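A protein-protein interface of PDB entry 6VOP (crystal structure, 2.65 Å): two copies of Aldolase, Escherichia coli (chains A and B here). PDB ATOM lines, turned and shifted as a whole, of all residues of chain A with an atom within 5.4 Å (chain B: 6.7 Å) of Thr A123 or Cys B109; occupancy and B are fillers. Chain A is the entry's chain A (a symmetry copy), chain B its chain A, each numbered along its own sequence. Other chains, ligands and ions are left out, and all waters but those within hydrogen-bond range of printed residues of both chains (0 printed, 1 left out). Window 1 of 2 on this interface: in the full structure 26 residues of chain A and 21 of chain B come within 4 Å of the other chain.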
ATOM      1  N   PRO A 121      13.060   1.024  16.507  1.00  0.00           N
ATOM      2  CA  PRO A 121      12.707   1.765  15.286  1.00  0.00           C
ATOM      3  C   PRO A 121      13.271   1.123  14.025  1.00  0.00           C
ATOM      4  O   PRO A 121      14.465   0.828  13.936  1.00  0.00           O
ATOM      5  CB  PRO A 121      13.312   3.152  15.526  1.00  0.00           C
ATOM      6  CG  PRO A 121      14.384   2.935  16.529  1.00  0.00           C
ATOM      7  CD  PRO A 121      13.924   1.808  17.403  1.00  0.00           C
ATOM      8  N   PHE A 122      12.384   0.906  13.049  1.00  0.00           N
ATOM      9  CA  PHE A 122      12.759   0.592  11.679  1.00  0.00           C
ATOM     10  C   PHE A 122      12.264   1.633  10.684  1.00  0.00           C
ATOM     11  O   PHE A 122      12.600   1.541   9.498  1.00  0.00           O
ATOM     12  CB  PHE A 122      12.223  -0.789  11.269  1.00  0.00           C
ATOM     13  CG  PHE A 122      10.805  -1.034  11.687  1.00  0.00           C
ATOM     14  CD1 PHE A 122       9.753  -0.624  10.887  1.00  0.00           C
ATOM     15  CD2 PHE A 122      10.524  -1.672  12.883  1.00  0.00           C
ATOM     16  CE1 PHE A 122       8.445  -0.849  11.270  1.00  0.00           C
ATOM     17  CE2 PHE A 122       9.218  -1.898  13.273  1.00  0.00           C
ATOM     18  CZ  PHE A 122       8.176  -1.487  12.466  1.00  0.00           C
ATOM     19  N   THR A 123      11.460   2.599  11.129  1.00  0.00           N
ATOM     20  CA  THR A 123      11.056   3.797  10.414  1.00  0.00           C
ATOM     21  C   THR A 123      11.412   5.016  11.257  1.00  0.00           C
ATOM     22  O   THR A 123      11.391   4.945  12.490  1.00  0.00           O
ATOM     23  CB  THR A 123       9.551   3.811  10.110  1.00  0.00           C
ATOM     24  OG1 THR A 123       8.811   3.634  11.325  1.00  0.00           O
ATOM     25  CG2 THR A 123       9.189   2.707   9.127  1.00  0.00           C
ATOM     26  N   PRO A 124      11.742   6.148  10.628  1.00  0.00           N
ATOM     27  CA  PRO A 124      12.271   7.285  11.394  1.00  0.00           C
ATOM     28  C   PRO A 124      11.220   8.133  12.093  1.00  0.00           C
ATOM     29  O   PRO A 124      11.590   8.997  12.898  1.00  0.00           O
ATOM     30  CB  PRO A 124      12.993   8.106  10.322  1.00  0.00           C
ATOM     31  CG  PRO A 124      12.186   7.859   9.093  1.00  0.00           C
ATOM     32  CD  PRO A 124      11.716   6.427   9.181  1.00  0.00           C
ATOM     33  N   TYR A 125       9.932   7.910  11.838  1.00  0.00           N
ATOM     34  CA  TYR A 125       8.941   8.931  12.160  1.00  0.00           C
ATOM     35  C   TYR A 125       8.569   8.948  13.639  1.00  0.00           C
ATOM     36  O   TYR A 125       8.414  10.026  14.222  1.00  0.00           O
ATOM     37  CB  TYR A 125       7.710   8.740  11.275  1.00  0.00           C
ATOM     38  CG  TYR A 125       8.056   8.884   9.811  1.00  0.00           C
ATOM     39  CD1 TYR A 125       8.327  10.133   9.267  1.00  0.00           C
ATOM     40  CD2 TYR A 125       8.153   7.771   8.983  1.00  0.00           C
ATOM     41  CE1 TYR A 125       8.663  10.276   7.937  1.00  0.00           C
ATOM     42  CE2 TYR A 125       8.489   7.902   7.648  1.00  0.00           C
ATOM     43  CZ  TYR A 125       8.744   9.159   7.133  1.00  0.00           C
ATOM     44  OH  TYR A 125       9.077   9.303   5.805  1.00  0.00           O
ATOM     45  N   VAL A 126       8.434   7.779  14.269  1.00  0.00           N
ATOM     46  CA  VAL A 126       8.058   7.767  15.681  1.00  0.00           C
ATOM     47  C   VAL A 126       9.197   8.292  16.552  1.00  0.00           C
ATOM     48  O   VAL A 126       8.954   8.928  17.585  1.00  0.00           O
ATOM     49  CB  VAL A 126       7.613   6.354  16.100  1.00  0.00           C
ATOM     50  CG1 VAL A 126       7.281   6.308  17.583  1.00  0.00           C
ATOM     51  CG2 VAL A 126       6.404   5.944  15.295  1.00  0.00           C
ATOM     52  N   VAL A 127      10.446   8.060  16.152  1.00  0.00           N
ATOM     53  CA  VAL A 127      11.574   8.613  16.897  1.00  0.00           C
ATOM     54  C   VAL A 127      11.618  10.130  16.750  1.00  0.00           C
ATOM     55  O   VAL A 127      11.945  10.851  17.701  1.00  0.00           O
ATOM     56  CB  VAL A 127      12.888   7.957  16.435  1.00  0.00           C
ATOM     57  CG1 VAL A 127      14.073   8.564  17.168  1.00  0.00           C
ATOM     58  CG2 VAL A 127      12.830   6.460  16.661  1.00  0.00           C
ATOM     59  N   GLU A 183       0.793   7.646  13.969  1.00  0.00           N
ATOM     60  CA  GLU A 183       2.085   7.082  13.590  1.00  0.00           C
ATOM     61  C   GLU A 183       2.545   6.000  14.561  1.00  0.00           C
ATOM     62  O   GLU A 183       3.272   5.082  14.161  1.00  0.00           O
ATOM     63  CB  GLU A 183       3.141   8.186  13.490  1.00  0.00           C
ATOM     64  CG  GLU A 183       4.410   7.769  12.752  1.00  0.00           C
ATOM     65  CD  GLU A 183       4.246   7.785  11.242  1.00  0.00           C
ATOM     66  OE1 GLU A 183       4.588   6.773  10.594  1.00  0.00           O
ATOM     67  OE2 GLU A 183       3.777   8.810  10.703  1.00  0.00           O
ATOM     68  N   THR A 187       3.139   2.139  13.439  1.00  0.00           N
ATOM     69  CA  THR A 187       4.394   1.431  13.658  1.00  0.00           C
ATOM     70  C   THR A 187       4.161   0.081  14.325  1.00  0.00           C
ATOM     71  O   THR A 187       4.796  -0.915  13.956  1.00  0.00           O
ATOM     72  CB  THR A 187       5.342   2.295  14.485  1.00  0.00           C
ATOM     73  OG1 THR A 187       5.754   3.417  13.698  1.00  0.00           O
ATOM     74  CG2 THR A 187       6.572   1.503  14.906  1.00  0.00           C
ATOM     75  N   LEU A 190       3.107  -2.240  11.679  1.00  0.00           N
ATOM     76  CA  LEU A 190       4.203  -2.761  10.869  1.00  0.00           C
ATOM     77  C   LEU A 190       4.962  -3.862  11.596  1.00  0.00           C
ATOM     78  O   LEU A 190       5.460  -4.795  10.955  1.00  0.00           O
ATOM     79  CB  LEU A 190       5.156  -1.635  10.480  1.00  0.00           C
ATOM     80  CG  LEU A 190       4.564  -0.547   9.587  1.00  0.00           C
ATOM     81  CD1 LEU A 190       5.643   0.432   9.155  1.00  0.00           C
ATOM     82  CD2 LEU A 190       3.883  -1.171   8.383  1.00  0.00           C
ATOM     83  N   LEU A 194       5.533  -7.280   9.666  1.00  0.00           N
ATOM     84  CA  LEU A 194       6.868  -7.782   9.358  1.00  0.00           C
ATOM     85  C   LEU A 194       7.115  -9.127  10.030  1.00  0.00           C
ATOM     86  O   LEU A 194       7.673 -10.042   9.412  1.00  0.00           O
ATOM     87  CB  LEU A 194       7.919  -6.754   9.776  1.00  0.00           C
ATOM     88  CG  LEU A 194       7.882  -5.463   8.953  1.00  0.00           C
ATOM     89  CD1 LEU A 194       8.698  -4.352   9.602  1.00  0.00           C
ATOM     90  CD2 LEU A 194       8.360  -5.725   7.535  1.00  0.00           C
ATOM     91  N   PRO A 198      13.439 -10.873   8.312  1.00  0.00           N
ATOM     92  CA  PRO A 198      14.631 -10.070   8.617  1.00  0.00           C
ATOM     93  C   PRO A 198      14.425  -8.593   8.314  1.00  0.00           C
ATOM     94  O   PRO A 198      14.484  -8.169   7.154  1.00  0.00           O
ATOM     95  CB  PRO A 198      15.714 -10.688   7.722  1.00  0.00           C
ATOM     96  CG  PRO A 198      14.964 -11.386   6.634  1.00  0.00           C
ATOM     97  CD  PRO A 198      13.698 -11.876   7.265  1.00  0.00           C
ATOM     98  N   ILE A 199      14.180  -7.806   9.356  1.00  0.00           N
ATOM     99  CA  ILE A 199      13.927  -6.375   9.228  1.00  0.00           C
ATOM    100  C   ILE A 199      15.254  -5.634   9.197  1.00  0.00           C
ATOM    101  O   ILE A 199      16.206  -6.003   9.897  1.00  0.00           O
ATOM    102  CB  ILE A 199      13.040  -5.875  10.384  1.00  0.00           C
ATOM    103  CG1 ILE A 199      11.807  -6.764  10.533  1.00  0.00           C
ATOM    104  CG2 ILE A 199      12.626  -4.428  10.160  1.00  0.00           C
ATOM    105  CD1 ILE A 199      11.009  -6.478  11.780  1.00  0.00           C
ATOM    106  N   ARG A 200      15.323  -4.584   8.380  1.00  0.00           N
ATOM    107  CA  ARG A 200      16.477  -3.687   8.360  1.00  0.00           C
ATOM    108  C   ARG A 200      16.192  -2.547   9.329  1.00  0.00           C
ATOM    109  O   ARG A 200      15.678  -1.491   8.955  1.00  0.00           O
ATOM    110  CB  ARG A 200      16.753  -3.174   6.953  1.00  0.00           C
ATOM    111  CG  ARG A 200      18.130  -2.548   6.795  1.00  0.00           C
ATOM    112  CD  ARG A 200      18.089  -1.317   5.909  1.00  0.00           C
ATOM    113  NE  ARG A 200      17.706  -0.117   6.648  1.00  0.00           N
ATOM    114  CZ  ARG A 200      18.568   0.712   7.229  1.00  0.00           C
ATOM    115  NH1 ARG A 200      19.871   0.472   7.161  1.00  0.00           N
ATOM    116  NH2 ARG A 200      18.130   1.782   7.878  1.00  0.00           N
ATOM    117  N   LEU A 202      16.821   0.611  11.811  1.00  0.00           N
ATOM    118  CA  LEU A 202      17.691   1.778  11.784  1.00  0.00           C
ATOM    119  C   LEU A 202      18.851   1.567  12.747  1.00  0.00           C
ATOM    120  O   LEU A 202      18.649   1.174  13.901  1.00  0.00           O
ATOM    121  CB  LEU A 202      16.911   3.039  12.158  1.00  0.00           C
ATOM    122  CG  LEU A 202      15.639   3.372  11.372  1.00  0.00           C
ATOM    123  CD1 LEU A 202      15.078   4.709  11.827  1.00  0.00           C
ATOM    124  CD2 LEU A 202      15.889   3.381   9.871  1.00  0.00           C
ATOM    125  N   SER B 104       3.234  -0.991   1.665  1.00  0.00           N
ATOM    126  CA  SER B 104       4.393  -0.551   0.895  1.00  0.00           C
ATOM    127  C   SER B 104       5.526  -0.126   1.819  1.00  0.00           C
ATOM    128  O   SER B 104       6.691  -0.467   1.579  1.00  0.00           O
ATOM    129  CB  SER B 104       4.001   0.592  -0.037  1.00  0.00           C
ATOM    130  OG  SER B 104       2.768   0.322  -0.669  1.00  0.00           O
ATOM    131  N   THR B 105       5.199   0.615   2.884  1.00  0.00           N
ATOM    132  CA  THR B 105       6.213   0.981   3.866  1.00  0.00           C
ATOM    133  C   THR B 105       6.767  -0.256   4.560  1.00  0.00           C
ATOM    134  O   THR B 105       7.963  -0.319   4.869  1.00  0.00           O
ATOM    135  CB  THR B 105       5.634   1.954   4.894  1.00  0.00           C
ATOM    136  OG1 THR B 105       4.952   3.022   4.223  1.00  0.00           O
ATOM    137  CG2 THR B 105       6.745   2.536   5.756  1.00  0.00           C
ATOM    138  N   ALA B 106       5.914  -1.253   4.810  1.00  0.00           N
ATOM    139  CA  ALA B 106       6.391  -2.497   5.406  1.00  0.00           C
ATOM    140  C   ALA B 106       7.383  -3.196   4.485  1.00  0.00           C
ATOM    141  O   ALA B 106       8.467  -3.608   4.917  1.00  0.00           O
ATOM    142  CB  ALA B 106       5.210  -3.414   5.727  1.00  0.00           C
ATOM    143  N   LEU B 107       7.030  -3.333   3.204  1.00  0.00           N
ATOM    144  CA  LEU B 107       7.935  -3.967   2.251  1.00  0.00           C
ATOM    145  C   LEU B 107       9.281  -3.254   2.208  1.00  0.00           C
ATOM    146  O   LEU B 107      10.331  -3.903   2.151  1.00  0.00           O
ATOM    147  CB  LEU B 107       7.296  -3.999   0.862  1.00  0.00           C
ATOM    148  CG  LEU B 107       8.091  -4.685  -0.256  1.00  0.00           C
ATOM    149  CD1 LEU B 107       8.025  -6.202  -0.138  1.00  0.00           C
ATOM    150  CD2 LEU B 107       7.596  -4.229  -1.621  1.00  0.00           C
ATOM    151  N   SER B 108       9.271  -1.921   2.268  1.00  0.00           N
ATOM    152  CA  SER B 108      10.498  -1.137   2.170  1.00  0.00           C
ATOM    153  C   SER B 108      11.434  -1.322   3.359  1.00  0.00           C
ATOM    154  O   SER B 108      12.564  -0.827   3.311  1.00  0.00           O
ATOM    155  CB  SER B 108      10.158   0.347   2.017  1.00  0.00           C
ATOM    156  OG  SER B 108       9.582   0.868   3.202  1.00  0.00           O
ATOM    157  N   CYS B 109      11.000  -2.006   4.418  1.00  0.00           N
ATOM    158  CA  CYS B 109      11.820  -2.234   5.600  1.00  0.00           C
ATOM    159  C   CYS B 109      12.473  -3.610   5.606  1.00  0.00           C
ATOM    160  O   CYS B 109      13.019  -4.020   6.637  1.00  0.00           O
ATOM    161  CB  CYS B 109      10.986  -2.069   6.871  1.00  0.00           C
ATOM    162  SG  CYS B 109      10.247  -0.449   7.103  1.00  0.00           S
ATOM    163  N   LEU B 110      12.423  -4.332   4.493  1.00  0.00           N
ATOM    164  CA  LEU B 110      12.918  -5.698   4.445  1.00  0.00           C
ATOM    165  C   LEU B 110      14.364  -5.734   3.968  1.00  0.00           C
ATOM    166  O   LEU B 110      14.758  -4.976   3.077  1.00  0.00           O
ATOM    167  CB  LEU B 110      12.042  -6.550   3.525  1.00  0.00           C
ATOM    168  CG  LEU B 110      10.614  -6.806   4.011  1.00  0.00           C
ATOM    169  CD1 LEU B 110       9.823  -7.575   2.965  1.00  0.00           C
ATOM    170  CD2 LEU B 110      10.629  -7.558   5.332  1.00  0.00           C
ATOM    171  N   GLN B 111      15.154  -6.612   4.583  1.00  0.00           N
ATOM    172  CA  GLN B 111      16.502  -6.864   4.107  1.00  0.00           C
ATOM    173  C   GLN B 111      16.462  -7.692   2.826  1.00  0.00           C
ATOM    174  O   GLN B 111      15.493  -8.403   2.541  1.00  0.00           O
ATOM    175  CB  GLN B 111      17.330  -7.603   5.160  1.00  0.00           C
ATOM    176  CG  GLN B 111      17.468  -6.896   6.495  1.00  0.00           C
ATOM    177  CD  GLN B 111      18.223  -7.736   7.516  1.00  0.00           C
ATOM    178  OE1 GLN B 111      19.005  -8.617   7.155  1.00  0.00           O
ATOM    179  NE2 GLN B 111      17.984  -7.474   8.798  1.00  0.00           N
ATOM    180  N   LEU B 113      16.159  -6.844  -0.263  1.00  0.00           N
ATOM    181  CA  LEU B 113      15.288  -6.429  -1.349  1.00  0.00           C
ATOM    182  C   LEU B 113      16.086  -6.247  -2.638  1.00  0.00           C
ATOM    183  O   LEU B 113      17.310  -6.077  -2.630  1.00  0.00           O
ATOM    184  CB  LEU B 113      14.572  -5.124  -0.996  1.00  0.00           C
ATOM    185  CG  LEU B 113      13.253  -5.250  -0.236  1.00  0.00           C
ATOM    186  CD1 LEU B 113      12.521  -3.916  -0.214  1.00  0.00           C
ATOM    187  CD2 LEU B 113      12.390  -6.337  -0.852  1.00  0.00           C
ATOM    188  N   TYR B 138      17.893   4.403   2.080  1.00  0.00           N
ATOM    189  CA  TYR B 138      17.396   5.130   3.239  1.00  0.00           C
ATOM    190  C   TYR B 138      18.308   6.307   3.555  1.00  0.00           C
ATOM    191  O   TYR B 138      19.529   6.150   3.662  1.00  0.00           O
ATOM    192  CB  TYR B 138      17.284   4.229   4.470  1.00  0.00           C
ATOM    193  CG  TYR B 138      17.090   5.042   5.734  1.00  0.00           C
ATOM    194  CD1 TYR B 138      15.873   5.662   6.003  1.00  0.00           C
ATOM    195  CD2 TYR B 138      18.129   5.226   6.635  1.00  0.00           C
ATOM    196  CE1 TYR B 138      15.692   6.425   7.141  1.00  0.00           C
ATOM    197  CE2 TYR B 138      17.958   5.988   7.777  1.00  0.00           C
ATOM    198  CZ  TYR B 138      16.737   6.584   8.026  1.00  0.00           C
ATOM    199  OH  TYR B 138      16.562   7.341   9.161  1.00  0.00           O
ATOM    200  N   LEU B 161      10.303   2.933  -4.429  1.00  0.00           N
ATOM    201  CA  LEU B 161      10.124   2.529  -3.038  1.00  0.00           C
ATOM    202  C   LEU B 161      11.318   3.024  -2.232  1.00  0.00           C
ATOM    203  O   LEU B 161      12.437   2.530  -2.401  1.00  0.00           O
ATOM    204  CB  LEU B 161       9.969   1.015  -2.916  1.00  0.00           C
ATOM    205  CG  LEU B 161       9.525   0.540  -1.531  1.00  0.00           C
ATOM    206  CD1 LEU B 161       8.169   1.128  -1.171  1.00  0.00           C
ATOM    207  CD2 LEU B 161       9.492  -0.975  -1.465  1.00  0.00           C
ATOM    208  N   LEU B 162      11.075   3.996  -1.356  1.00  0.00           N
ATOM    209  CA  LEU B 162      12.113   4.552  -0.496  1.00  0.00           C
ATOM    210  C   LEU B 162      12.234   3.685   0.752  1.00  0.00           C
ATOM    211  O   LEU B 162      11.251   3.490   1.474  1.00  0.00           O
ATOM    212  CB  LEU B 162      11.787   5.996  -0.120  1.00  0.00           C
ATOM    213  CG  LEU B 162      12.139   7.111  -1.109  1.00  0.00           C
ATOM    214  CD1 LEU B 162      11.407   6.934  -2.427  1.00  0.00           C
ATOM    215  CD2 LEU B 162      11.819   8.470  -0.503  1.00  0.00           C
ATOM    216  N   ALA B 163      13.439   3.177   1.006  1.00  0.00           N
ATOM    217  CA  ALA B 163      13.650   2.229   2.093  1.00  0.00           C
ATOM    218  C   ALA B 163      13.367   2.866   3.447  1.00  0.00           C
ATOM    219  O   ALA B 163      13.743   4.013   3.707  1.00  0.00           O
ATOM    220  CB  ALA B 163      15.083   1.698   2.055  1.00  0.00           C
ATOM    221  N   ASN B 164      12.701   2.101   4.316  1.00  0.00           N
ATOM    222  CA  ASN B 164      12.322   2.562   5.653  1.00  0.00           C
ATOM    223  C   ASN B 164      11.555   3.879   5.581  1.00  0.00           C
ATOM    224  O   ASN B 164      11.695   4.755   6.438  1.00  0.00           O
ATOM    225  CB  ASN B 164      13.549   2.689   6.561  1.00  0.00           C
ATOM    226  CG  ASN B 164      14.364   1.409   6.628  1.00  0.00           C
ATOM    227  OD1 ASN B 164      15.225   1.165   5.782  1.00  0.00           O
ATOM    228  ND2 ASN B 164      14.101   0.588   7.640  1.00  0.00           N
ATOM    229  N   HIS B 165      10.731   4.019   4.544  1.00  0.00           N
ATOM    230  CA  HIS B 165      10.066   5.284   4.255  1.00  0.00           C
ATOM    231  C   HIS B 165       8.697   5.047   3.625  1.00  0.00           C
ATOM    232  O   HIS B 165       7.666   5.340   4.241  1.00  0.00           O
ATOM    233  CB  HIS B 165      10.946   6.134   3.336  1.00  0.00           C
ATOM    234  CG  HIS B 165      10.478   7.547   3.174  1.00  0.00           C
ATOM    235  ND1 HIS B 165      11.341   8.621   3.213  1.00  0.00           N
ATOM    236  CD2 HIS B 165       9.246   8.063   2.954  1.00  0.00           C
ATOM    237  CE1 HIS B 165      10.660   9.738   3.034  1.00  0.00           C
ATOM    238  NE2 HIS B 165       9.386   9.428   2.876  1.00  0.00           N
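Printed residues of chain B within 4 Å of Phe A122: Cys B109 (3.8 Å) and Asn B164 (2.6 Å).
Thr A123 touches one residue of chain B.
Val A127 touches none of the printed residues of chain B.
Of the printed residues of chain B, Arg A200 touches Cys B109 (2.9 Å), Gln B111 (3.7 Å), Tyr B138 (3.7 Å) and Asn B164 (2.9 Å).
Of the printed residues of chain B, Leu A202 touches Tyr B138 and Asn B164.
Cys B109 touches just these residues of chain A: Phe A122, Thr A123, Ile A199 and Arg A200.
Of the printed residues of chain A, Leu B110 touches Leu A194 (3.7 Å) and Pro A198 (3.99 Å).
Of the printed residues of chain A, Tyr B138 touches Pro A124 (3.8 Å), Arg A200 (3.7 Å) and Leu A202 (3.8 Å).
The nearest printed residue of chain B that does not touch Arg A200 is Leu B110 (4.6 Å).
No position is printed for both chains.
Of the 19 pairs that touch across the chains among the printed residues, none has its exchanged pair printed and touching as well.
The backbone carbonyl oxygen of Pro A198 lies within hydrogen-bond range of the backbone NH of Gln B111 (3.1 Å).
The side-chain amide nitrogen of Gln B111 lies within hydrogen-bond range of the backbone carbonyl oxygen of Ile A199, at 2.6 Å.
The side-chain amide nitrogen (ND2) of Asn B164 lies within hydrogen-bond range of the backbone carbonyl oxygen (O) of Arg A200 (2.9 Å).
O of Cys B109 is in hydrogen-bond range of N of Arg A200, 2.9 Å away.
NE2 of His B165 lies within hydrogen-bond range of OH of Tyr A125, at 2.9 Å.
The side-chain amide nitrogen (ND2) of Asn B164 is in hydrogen-bond range of the backbone carbonyl oxygen (O) of Phe A122 (2.6 Å).
O of Ser B108 lies within hydrogen-bond range of N of Asn B164.
The backbone carbonyl oxygen (O) of Thr B105 is in hydrogen-bond range of the side-chain sulfur (SG) of Cys B109, at 3.2 Å.
O of Pro A121 is in hydrogen-bond range of N of Leu A202, 3.2 Å away.
Printed residues of chain B that touch a printed residue of chain A: Ala B106, Cys B109, Leu B110, Gln B111, Tyr B138, Asn B164 and His B165.
Hydrophobic or aromatic side chains of chain B within 4 Å of the printed part of chain A: Ala B106, Leu B110, Tyr B138 and His B165.
Of the 15 printed residues of chain A, 10 touch a printed residue of chain B.
Printed residues of chain A that touch a printed residue of chain B: Phe A122, Thr A123, Pro A124, Tyr A125, Leu A190, Leu A194, Pro A198, Ile A199, Arg A200 and Leu A202.
Hydrophobic or aromatic side chains of chain A within 4 Å of the printed part of chain B: Phe A122, Pro A124, Tyr A125, Leu A190, Leu A194, Pro A198, Ile A199 and Leu A202.
Among the printed residues, 19 pairs touch across the chains.
Phe A122 touches Cys B109 (CD1 to SG, 3.8 Å).
CD of Pro A124 touches O of Asn B164, at 3.2 Å.
Leu A190 touches Ala B106.
Ala B106 touches Leu A194 (O to CD2, 3.4 Å).
Leu B110 touches Leu A194 (CD2 to CD2, 3.7 Å).
Leu B110 touches Pro A198.
Ile A199 touches Cys B109 (CG2 to O, 3.6 Å).
Arg A200 touches Tyr B138.
Leu A202 touches Tyr B138 (CD2 to CZ, 3.8 Å).
Asn B164 touches Leu A202.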
